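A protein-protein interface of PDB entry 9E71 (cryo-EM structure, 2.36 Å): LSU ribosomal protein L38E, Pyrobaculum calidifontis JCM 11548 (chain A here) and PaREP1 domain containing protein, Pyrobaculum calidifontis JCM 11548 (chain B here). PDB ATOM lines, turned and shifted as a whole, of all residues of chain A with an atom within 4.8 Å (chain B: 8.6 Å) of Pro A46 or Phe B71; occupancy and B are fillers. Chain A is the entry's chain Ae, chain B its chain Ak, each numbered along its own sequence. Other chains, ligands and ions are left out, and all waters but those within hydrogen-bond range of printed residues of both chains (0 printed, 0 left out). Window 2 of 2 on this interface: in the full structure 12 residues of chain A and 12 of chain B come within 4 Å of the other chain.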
ATOM      1  N   ASP A  28      -7.562 -18.227   6.045  1.00  0.00           N
ATOM      2  CA  ASP A  28      -6.643 -17.244   5.487  1.00  0.00           C
ATOM      3  C   ASP A  28      -6.266 -17.494   4.035  1.00  0.00           C
ATOM      4  O   ASP A  28      -5.792 -16.567   3.373  1.00  0.00           O
ATOM      5  CB  ASP A  28      -5.348 -17.176   6.308  1.00  0.00           C
ATOM      6  CG  ASP A  28      -5.586 -17.318   7.786  1.00  0.00           C
ATOM      7  OD1 ASP A  28      -5.604 -18.466   8.270  1.00  0.00           O
ATOM      8  OD2 ASP A  28      -5.760 -16.285   8.465  1.00  0.00           O
ATOM      9  N   PHE A  29      -6.445 -18.706   3.524  1.00  0.00           N
ATOM     10  CA  PHE A  29      -5.922 -19.001   2.199  1.00  0.00           C
ATOM     11  C   PHE A  29      -6.740 -20.105   1.554  1.00  0.00           C
ATOM     12  O   PHE A  29      -7.432 -20.876   2.223  1.00  0.00           O
ATOM     13  CB  PHE A  29      -4.437 -19.386   2.258  1.00  0.00           C
ATOM     14  CG  PHE A  29      -4.157 -20.647   3.030  1.00  0.00           C
ATOM     15  CD1 PHE A  29      -4.050 -20.626   4.409  1.00  0.00           C
ATOM     16  CD2 PHE A  29      -3.981 -21.851   2.373  1.00  0.00           C
ATOM     17  CE1 PHE A  29      -3.790 -21.782   5.114  1.00  0.00           C
ATOM     18  CE2 PHE A  29      -3.719 -23.008   3.075  1.00  0.00           C
ATOM     19  CZ  PHE A  29      -3.623 -22.973   4.446  1.00  0.00           C
ATOM     20  N   ARG A  44      -1.262 -21.934  -2.965  1.00  0.00           N
ATOM     21  CA  ARG A  44      -1.997 -21.310  -1.875  1.00  0.00           C
ATOM     22  C   ARG A  44      -2.080 -19.814  -2.138  1.00  0.00           C
ATOM     23  O   ARG A  44      -1.050 -19.150  -2.277  1.00  0.00           O
ATOM     24  CB  ARG A  44      -1.324 -21.580  -0.532  1.00  0.00           C
ATOM     25  CG  ARG A  44      -1.659 -22.924   0.073  1.00  0.00           C
ATOM     26  CD  ARG A  44      -0.406 -23.717   0.355  1.00  0.00           C
ATOM     27  NE  ARG A  44       0.286 -23.245   1.546  1.00  0.00           N
ATOM     28  CZ  ARG A  44       1.590 -23.017   1.606  1.00  0.00           C
ATOM     29  NH1 ARG A  44       2.373 -23.210   0.559  1.00  0.00           N
ATOM     30  NH2 ARG A  44       2.122 -22.585   2.745  1.00  0.00           N
ATOM     31  N   VAL A  45      -3.298 -19.286  -2.193  1.00  0.00           N
ATOM     32  CA  VAL A  45      -3.506 -17.882  -2.542  1.00  0.00           C
ATOM     33  C   VAL A  45      -4.401 -17.244  -1.492  1.00  0.00           C
ATOM     34  O   VAL A  45      -5.063 -17.942  -0.709  1.00  0.00           O
ATOM     35  CB  VAL A  45      -4.117 -17.730  -3.954  1.00  0.00           C
ATOM     36  CG1 VAL A  45      -3.223 -18.376  -4.987  1.00  0.00           C
ATOM     37  CG2 VAL A  45      -5.506 -18.334  -3.999  1.00  0.00           C
ATOM     38  N   PRO A  46      -4.428 -15.911  -1.433  1.00  0.00           N
ATOM     39  CA  PRO A  46      -5.421 -15.245  -0.594  1.00  0.00           C
ATOM     40  C   PRO A  46      -6.813 -15.488  -1.142  1.00  0.00           C
ATOM     41  O   PRO A  46      -6.975 -15.828  -2.325  1.00  0.00           O
ATOM     42  CB  PRO A  46      -5.031 -13.758  -0.688  1.00  0.00           C
ATOM     43  CG  PRO A  46      -3.794 -13.686  -1.483  1.00  0.00           C
ATOM     44  CD  PRO A  46      -3.598 -14.968  -2.196  1.00  0.00           C
ATOM     45  N   PRO A  47      -7.850 -15.377  -0.305  1.00  0.00           N
ATOM     46  CA  PRO A  47      -9.213 -15.696  -0.772  1.00  0.00           C
ATOM     47  C   PRO A  47      -9.721 -14.818  -1.908  1.00  0.00           C
ATOM     48  O   PRO A  47     -10.436 -15.313  -2.786  1.00  0.00           O
ATOM     49  CB  PRO A  47     -10.059 -15.530   0.497  1.00  0.00           C
ATOM     50  CG  PRO A  47      -9.102 -15.654   1.626  1.00  0.00           C
ATOM     51  CD  PRO A  47      -7.798 -15.119   1.141  1.00  0.00           C
ATOM     52  N   ASP A  48      -9.361 -13.533  -1.934  1.00  0.00           N
ATOM     53  CA  ASP A  48      -9.823 -12.664  -3.012  1.00  0.00           C
ATOM     54  C   ASP A  48      -9.183 -13.044  -4.344  1.00  0.00           C
ATOM     55  O   ASP A  48      -9.864 -13.123  -5.380  1.00  0.00           O
ATOM     56  CB  ASP A  48      -9.531 -11.206  -2.665  1.00  0.00           C
ATOM     57  CG  ASP A  48      -8.192 -11.032  -1.988  1.00  0.00           C
ATOM     58  OD1 ASP A  48      -7.379 -10.219  -2.474  1.00  0.00           O
ATOM     59  OD2 ASP A  48      -7.958 -11.704  -0.962  1.00  0.00           O
ATOM     60  N   LYS A  49      -7.870 -13.291  -4.332  1.00  0.00           N
ATOM     61  CA  LYS A  49      -7.198 -13.775  -5.531  1.00  0.00           C
ATOM     62  C   LYS A  49      -7.734 -15.138  -5.934  1.00  0.00           C
ATOM     63  O   LYS A  49      -7.818 -15.450  -7.125  1.00  0.00           O
ATOM     64  CB  LYS A  49      -5.689 -13.841  -5.301  1.00  0.00           C
ATOM     65  CG  LYS A  49      -4.848 -13.720  -6.562  1.00  0.00           C
ATOM     66  CD  LYS A  49      -4.567 -12.267  -6.886  1.00  0.00           C
ATOM     67  CE  LYS A  49      -3.906 -12.114  -8.240  1.00  0.00           C
ATOM     68  NZ  LYS A  49      -4.353 -13.154  -9.201  1.00  0.00           N
ATOM     69  N   ALA A  50      -8.114 -15.955  -4.951  1.00  0.00           N
ATOM     70  CA  ALA A  50      -8.726 -17.244  -5.244  1.00  0.00           C
ATOM     71  C   ALA A  50     -10.029 -17.063  -6.002  1.00  0.00           C
ATOM     72  O   ALA A  50     -10.267 -17.740  -7.004  1.00  0.00           O
ATOM     73  CB  ALA A  50      -8.961 -18.022  -3.952  1.00  0.00           C
ATOM     74  N   VAL B  35      10.491 -18.832   1.245  1.00  0.00           N
ATOM     75  CA  VAL B  35       9.308 -19.267   1.979  1.00  0.00           C
ATOM     76  C   VAL B  35       9.542 -20.621   2.632  1.00  0.00           C
ATOM     77  O   VAL B  35       9.159 -20.835   3.784  1.00  0.00           O
ATOM     78  CB  VAL B  35       8.078 -19.291   1.056  1.00  0.00           C
ATOM     79  CG1 VAL B  35       6.854 -19.738   1.835  1.00  0.00           C
ATOM     80  CG2 VAL B  35       7.848 -17.924   0.453  1.00  0.00           C
ATOM     81  N   LEU B  54      12.763 -13.453   6.940  1.00  0.00           N
ATOM     82  CA  LEU B  54      11.572 -12.707   6.544  1.00  0.00           C
ATOM     83  C   LEU B  54      11.911 -11.264   6.198  1.00  0.00           C
ATOM     84  O   LEU B  54      11.315 -10.688   5.284  1.00  0.00           O
ATOM     85  CB  LEU B  54      10.525 -12.760   7.653  1.00  0.00           C
ATOM     86  CG  LEU B  54       9.797 -14.096   7.786  1.00  0.00           C
ATOM     87  CD1 LEU B  54       8.444 -13.901   8.438  1.00  0.00           C
ATOM     88  CD2 LEU B  54       9.655 -14.756   6.429  1.00  0.00           C
ATOM     89  N   LYS B  58      11.298  -9.569   2.639  1.00  0.00           N
ATOM     90  CA  LYS B  58      10.656  -8.274   2.446  1.00  0.00           C
ATOM     91  C   LYS B  58      11.478  -7.392   1.518  1.00  0.00           C
ATOM     92  O   LYS B  58      10.938  -6.756   0.603  1.00  0.00           O
ATOM     93  CB  LYS B  58      10.443  -7.591   3.795  1.00  0.00           C
ATOM     94  CG  LYS B  58       9.177  -8.026   4.501  1.00  0.00           C
ATOM     95  CD  LYS B  58       9.339  -7.982   6.003  1.00  0.00           C
ATOM     96  CE  LYS B  58       8.694  -6.740   6.579  1.00  0.00           C
ATOM     97  NZ  LYS B  58       9.524  -5.529   6.327  1.00  0.00           N
ATOM     98  N   ALA B  61      11.151  -8.858  -2.028  1.00  0.00           N
ATOM     99  CA  ALA B  61       9.856  -8.560  -2.625  1.00  0.00           C
ATOM    100  C   ALA B  61       9.758  -7.100  -3.029  1.00  0.00           C
ATOM    101  O   ALA B  61       9.133  -6.783  -4.042  1.00  0.00           O
ATOM    102  CB  ALA B  61       8.729  -8.924  -1.662  1.00  0.00           C
ATOM    103  N   ILE B  66       7.060  -8.840  -5.984  1.00  0.00           N
ATOM    104  CA  ILE B  66       6.411 -10.137  -5.813  1.00  0.00           C
ATOM    105  C   ILE B  66       5.388 -10.015  -4.690  1.00  0.00           C
ATOM    106  O   ILE B  66       5.755  -9.795  -3.529  1.00  0.00           O
ATOM    107  CB  ILE B  66       7.423 -11.245  -5.515  1.00  0.00           C
ATOM    108  CG1 ILE B  66       8.344 -11.440  -6.715  1.00  0.00           C
ATOM    109  CG2 ILE B  66       6.705 -12.538  -5.177  1.00  0.00           C
ATOM    110  CD1 ILE B  66       9.718 -11.918  -6.341  1.00  0.00           C
ATOM    111  N   GLU B  67       4.105 -10.178  -5.032  1.00  0.00           N
ATOM    112  CA  GLU B  67       3.030 -10.071  -4.047  1.00  0.00           C
ATOM    113  C   GLU B  67       2.909 -11.347  -3.224  1.00  0.00           C
ATOM    114  O   GLU B  67       2.548 -11.285  -2.037  1.00  0.00           O
ATOM    115  CB  GLU B  67       1.722  -9.692  -4.786  1.00  0.00           C
ATOM    116  CG  GLU B  67       0.304  -9.579  -4.070  1.00  0.00           C
ATOM    117  CD  GLU B  67      -0.258 -10.788  -3.298  1.00  0.00           C
ATOM    118  OE1 GLU B  67      -1.111 -10.572  -2.409  1.00  0.00           O
ATOM    119  OE2 GLU B  67       0.053 -11.947  -3.642  1.00  0.00           O
ATOM    120  N   GLU B  68       3.170 -12.500  -3.843  1.00  0.00           N
ATOM    121  CA  GLU B  68       3.035 -13.770  -3.140  1.00  0.00           C
ATOM    122  C   GLU B  68       4.016 -13.862  -1.982  1.00  0.00           C
ATOM    123  O   GLU B  68       3.698 -14.437  -0.934  1.00  0.00           O
ATOM    124  CB  GLU B  68       3.241 -14.924  -4.115  1.00  0.00           C
ATOM    125  CG  GLU B  68       2.207 -14.983  -5.214  1.00  0.00           C
ATOM    126  CD  GLU B  68       2.659 -14.282  -6.480  1.00  0.00           C
ATOM    127  OE1 GLU B  68       3.452 -13.322  -6.391  1.00  0.00           O
ATOM    128  OE2 GLU B  68       2.229 -14.703  -7.571  1.00  0.00           O
ATOM    129  N   LEU B  69       5.208 -13.284  -2.151  1.00  0.00           N
ATOM    130  CA  LEU B  69       6.189 -13.264  -1.074  1.00  0.00           C
ATOM    131  C   LEU B  69       5.675 -12.475   0.120  1.00  0.00           C
ATOM    132  O   LEU B  69       5.808 -12.918   1.263  1.00  0.00           O
ATOM    133  CB  LEU B  69       7.507 -12.680  -1.573  1.00  0.00           C
ATOM    134  CG  LEU B  69       8.731 -12.969  -0.710  1.00  0.00           C
ATOM    135  CD1 LEU B  69       8.700 -14.409  -0.246  1.00  0.00           C
ATOM    136  CD2 LEU B  69       9.993 -12.684  -1.493  1.00  0.00           C
ATOM    137  N   ASN B  70       5.060 -11.315  -0.129  1.00  0.00           N
ATOM    138  CA  ASN B  70       4.493 -10.524   0.959  1.00  0.00           C
ATOM    139  C   ASN B  70       3.362 -11.267   1.657  1.00  0.00           C
ATOM    140  O   ASN B  70       3.258 -11.234   2.889  1.00  0.00           O
ATOM    141  CB  ASN B  70       4.000  -9.178   0.433  1.00  0.00           C
ATOM    142  CG  ASN B  70       5.083  -8.398  -0.271  1.00  0.00           C
ATOM    143  OD1 ASN B  70       4.880  -7.875  -1.367  1.00  0.00           O
ATOM    144  ND2 ASN B  70       6.249  -8.309   0.359  1.00  0.00           N
ATOM    145  N   PHE B  71       2.513 -11.947   0.886  1.00  0.00           N
ATOM    146  CA  PHE B  71       1.397 -12.686   1.477  1.00  0.00           C
ATOM    147  C   PHE B  71       1.892 -13.822   2.375  1.00  0.00           C
ATOM    148  O   PHE B  71       1.442 -13.979   3.523  1.00  0.00           O
ATOM    149  CB  PHE B  71       0.496 -13.205   0.354  1.00  0.00           C
ATOM    150  CG  PHE B  71      -0.557 -14.168   0.803  1.00  0.00           C
ATOM    151  CD1 PHE B  71      -1.499 -13.798   1.744  1.00  0.00           C
ATOM    152  CD2 PHE B  71      -0.622 -15.438   0.259  1.00  0.00           C
ATOM    153  CE1 PHE B  71      -2.473 -14.682   2.148  1.00  0.00           C
ATOM    154  CE2 PHE B  71      -1.592 -16.327   0.661  1.00  0.00           C
ATOM    155  CZ  PHE B  71      -2.520 -15.948   1.606  1.00  0.00           C
ATOM    156  N   HIS B  72       2.859 -14.598   1.885  1.00  0.00           N
ATOM    157  CA  HIS B  72       3.373 -15.707   2.678  1.00  0.00           C
ATOM    158  C   HIS B  72       4.170 -15.210   3.878  1.00  0.00           C
ATOM    159  O   HIS B  72       4.148 -15.832   4.948  1.00  0.00           O
ATOM    160  CB  HIS B  72       4.213 -16.627   1.796  1.00  0.00           C
ATOM    161  CG  HIS B  72       3.396 -17.486   0.883  1.00  0.00           C
ATOM    162  ND1 HIS B  72       2.642 -18.545   1.338  1.00  0.00           N
ATOM    163  CD2 HIS B  72       3.197 -17.433  -0.454  1.00  0.00           C
ATOM    164  CE1 HIS B  72       2.022 -19.112   0.320  1.00  0.00           C
ATOM    165  NE2 HIS B  72       2.340 -18.455  -0.779  1.00  0.00           N
ATOM    166  N   ILE B  73       4.864 -14.079   3.727  1.00  0.00           N
ATOM    167  CA  ILE B  73       5.586 -13.494   4.848  1.00  0.00           C
ATOM    168  C   ILE B  73       4.617 -13.031   5.922  1.00  0.00           C
ATOM    169  O   ILE B  73       4.892 -13.157   7.118  1.00  0.00           O
ATOM    170  CB  ILE B  73       6.481 -12.342   4.361  1.00  0.00           C
ATOM    171  CG1 ILE B  73       7.685 -12.893   3.604  1.00  0.00           C
ATOM    172  CG2 ILE B  73       6.943 -11.504   5.534  1.00  0.00           C
ATOM    173  CD1 ILE B  73       8.374 -11.863   2.745  1.00  0.00           C
ATOM    174  N   ALA B  74       3.472 -12.475   5.515  1.00  0.00           N
ATOM    175  CA  ALA B  74       2.465 -12.069   6.490  1.00  0.00           C
ATOM    176  C   ALA B  74       1.915 -13.269   7.250  1.00  0.00           C
ATOM    177  O   ALA B  74       1.714 -13.200   8.470  1.00  0.00           O
ATOM    178  CB  ALA B  74       1.339 -11.311   5.794  1.00  0.00           C
ATOM    179  N   LEU B  75       1.671 -14.379   6.547  1.00  0.00           N
ATOM    180  CA  LEU B  75       1.220 -15.595   7.227  1.00  0.00           C
ATOM    181  C   LEU B  75       2.261 -16.094   8.229  1.00  0.00           C
ATOM    182  O   LEU B  75       1.934 -16.440   9.375  1.00  0.00           O
ATOM    183  CB  LEU B  75       0.900 -16.681   6.201  1.00  0.00           C
ATOM    184  CG  LEU B  75      -0.277 -16.430   5.261  1.00  0.00           C
ATOM    185  CD1 LEU B  75      -0.386 -17.539   4.231  1.00  0.00           C
ATOM    186  CD2 LEU B  75      -1.565 -16.306   6.048  1.00  0.00           C
ATOM    187  N   LEU B  76       3.532 -16.112   7.817  1.00  0.00           N
ATOM    188  CA  LEU B  76       4.592 -16.566   8.711  1.00  0.00           C
ATOM    189  C   LEU B  76       4.768 -15.640   9.909  1.00  0.00           C
ATOM    190  O   LEU B  76       5.045 -16.111  11.016  1.00  0.00           O
ATOM    191  CB  LEU B  76       5.911 -16.697   7.948  1.00  0.00           C
ATOM    192  CG  LEU B  76       5.991 -17.620   6.729  1.00  0.00           C
ATOM    193  CD1 LEU B  76       7.378 -18.224   6.640  1.00  0.00           C
ATOM    194  CD2 LEU B  76       4.952 -18.725   6.788  1.00  0.00           C
ATOM    195  N   GLU B  77       4.611 -14.330   9.715  1.00  0.00           N
ATOM    196  CA  GLU B  77       4.746 -13.400  10.831  1.00  0.00           C
ATOM    197  C   GLU B  77       3.582 -13.533  11.800  1.00  0.00           C
ATOM    198  O   GLU B  77       3.759 -13.372  13.013  1.00  0.00           O
ATOM    199  CB  GLU B  77       4.864 -11.969  10.317  1.00  0.00           C
ATOM    200  CG  GLU B  77       6.104 -11.733   9.477  1.00  0.00           C
ATOM    201  CD  GLU B  77       6.989 -10.639  10.023  1.00  0.00           C
ATOM    202  OE1 GLU B  77       6.502  -9.502  10.182  1.00  0.00           O
ATOM    203  OE2 GLU B  77       8.176 -10.912  10.291  1.00  0.00           O
ATOM    204  N   LYS B  78       2.388 -13.839  11.287  1.00  0.00           N
ATOM    205  CA  LYS B  78       1.263 -14.151  12.163  1.00  0.00           C
ATOM    206  C   LYS B  78       1.561 -15.374  13.024  1.00  0.00           C
ATOM    207  O   LYS B  78       1.304 -15.380  14.238  1.00  0.00           O
ATOM    208  CB  LYS B  78       0.009 -14.376  11.321  1.00  0.00           C
ATOM    209  CG  LYS B  78      -1.142 -15.004  12.072  1.00  0.00           C
ATOM    210  CD  LYS B  78      -2.330 -15.202  11.158  1.00  0.00           C
ATOM    211  CE  LYS B  78      -2.586 -13.958  10.332  1.00  0.00           C
ATOM    212  NZ  LYS B  78      -2.702 -12.730  11.168  1.00  0.00           N
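Of the printed residues of chain B, Asp A28 touches Phe B71 (3.8 Å) and Leu B75 (3.9 Å). Pro A46 touches just one residue of chain B: Phe B71 (3.5 Å). Ala B61 touches none of the printed residues of chain A. Of the printed residues of chain A, Phe B71 touches Asp A28 (3.8 Å), Phe A29 (3.99 Å), Val A45 (3.7 Å) and Pro A46 (3.5 Å). Of the printed residues of chain A, His B72 touches Arg A44. The nearest printed residue of chain A that does not touch Phe B71 is Arg A44 (4.1 Å). The nearest printed residue of chain A that does not touch Leu B75 is Phe A29 (4.8 Å).
Printed residues of chain B that touch a printed residue of chain A: Phe B71, His B72 and Leu B75. Hydrophobic or aromatic side chains of chain B within 4 Å of the printed part of chain A: Phe B71, His B72 and Leu B75. Hydrophobic or aromatic side chains of chain A within 4 Å of the printed part of chain B: Phe A29 and Pro A46. Among the printed residues, 6 pairs touch across the chains. Among the printed residues, no Asp or Glu carboxylate lies within 4 Å of a Lys or Arg side-chain nitrogen of the other chain.
Among the printed residues, pairs that only touch across the chains: Pro A46 with Phe B71 (3.5 Å), Val A45 with Phe B71 (3.7 Å), Asp A28 with Phe B71 (3.8 Å), Arg A44 with His B72 (3.8 Å), Asp A28 with Leu B75 (3.9 Å) and Phe A29 with Phe B71 (3.99 Å).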
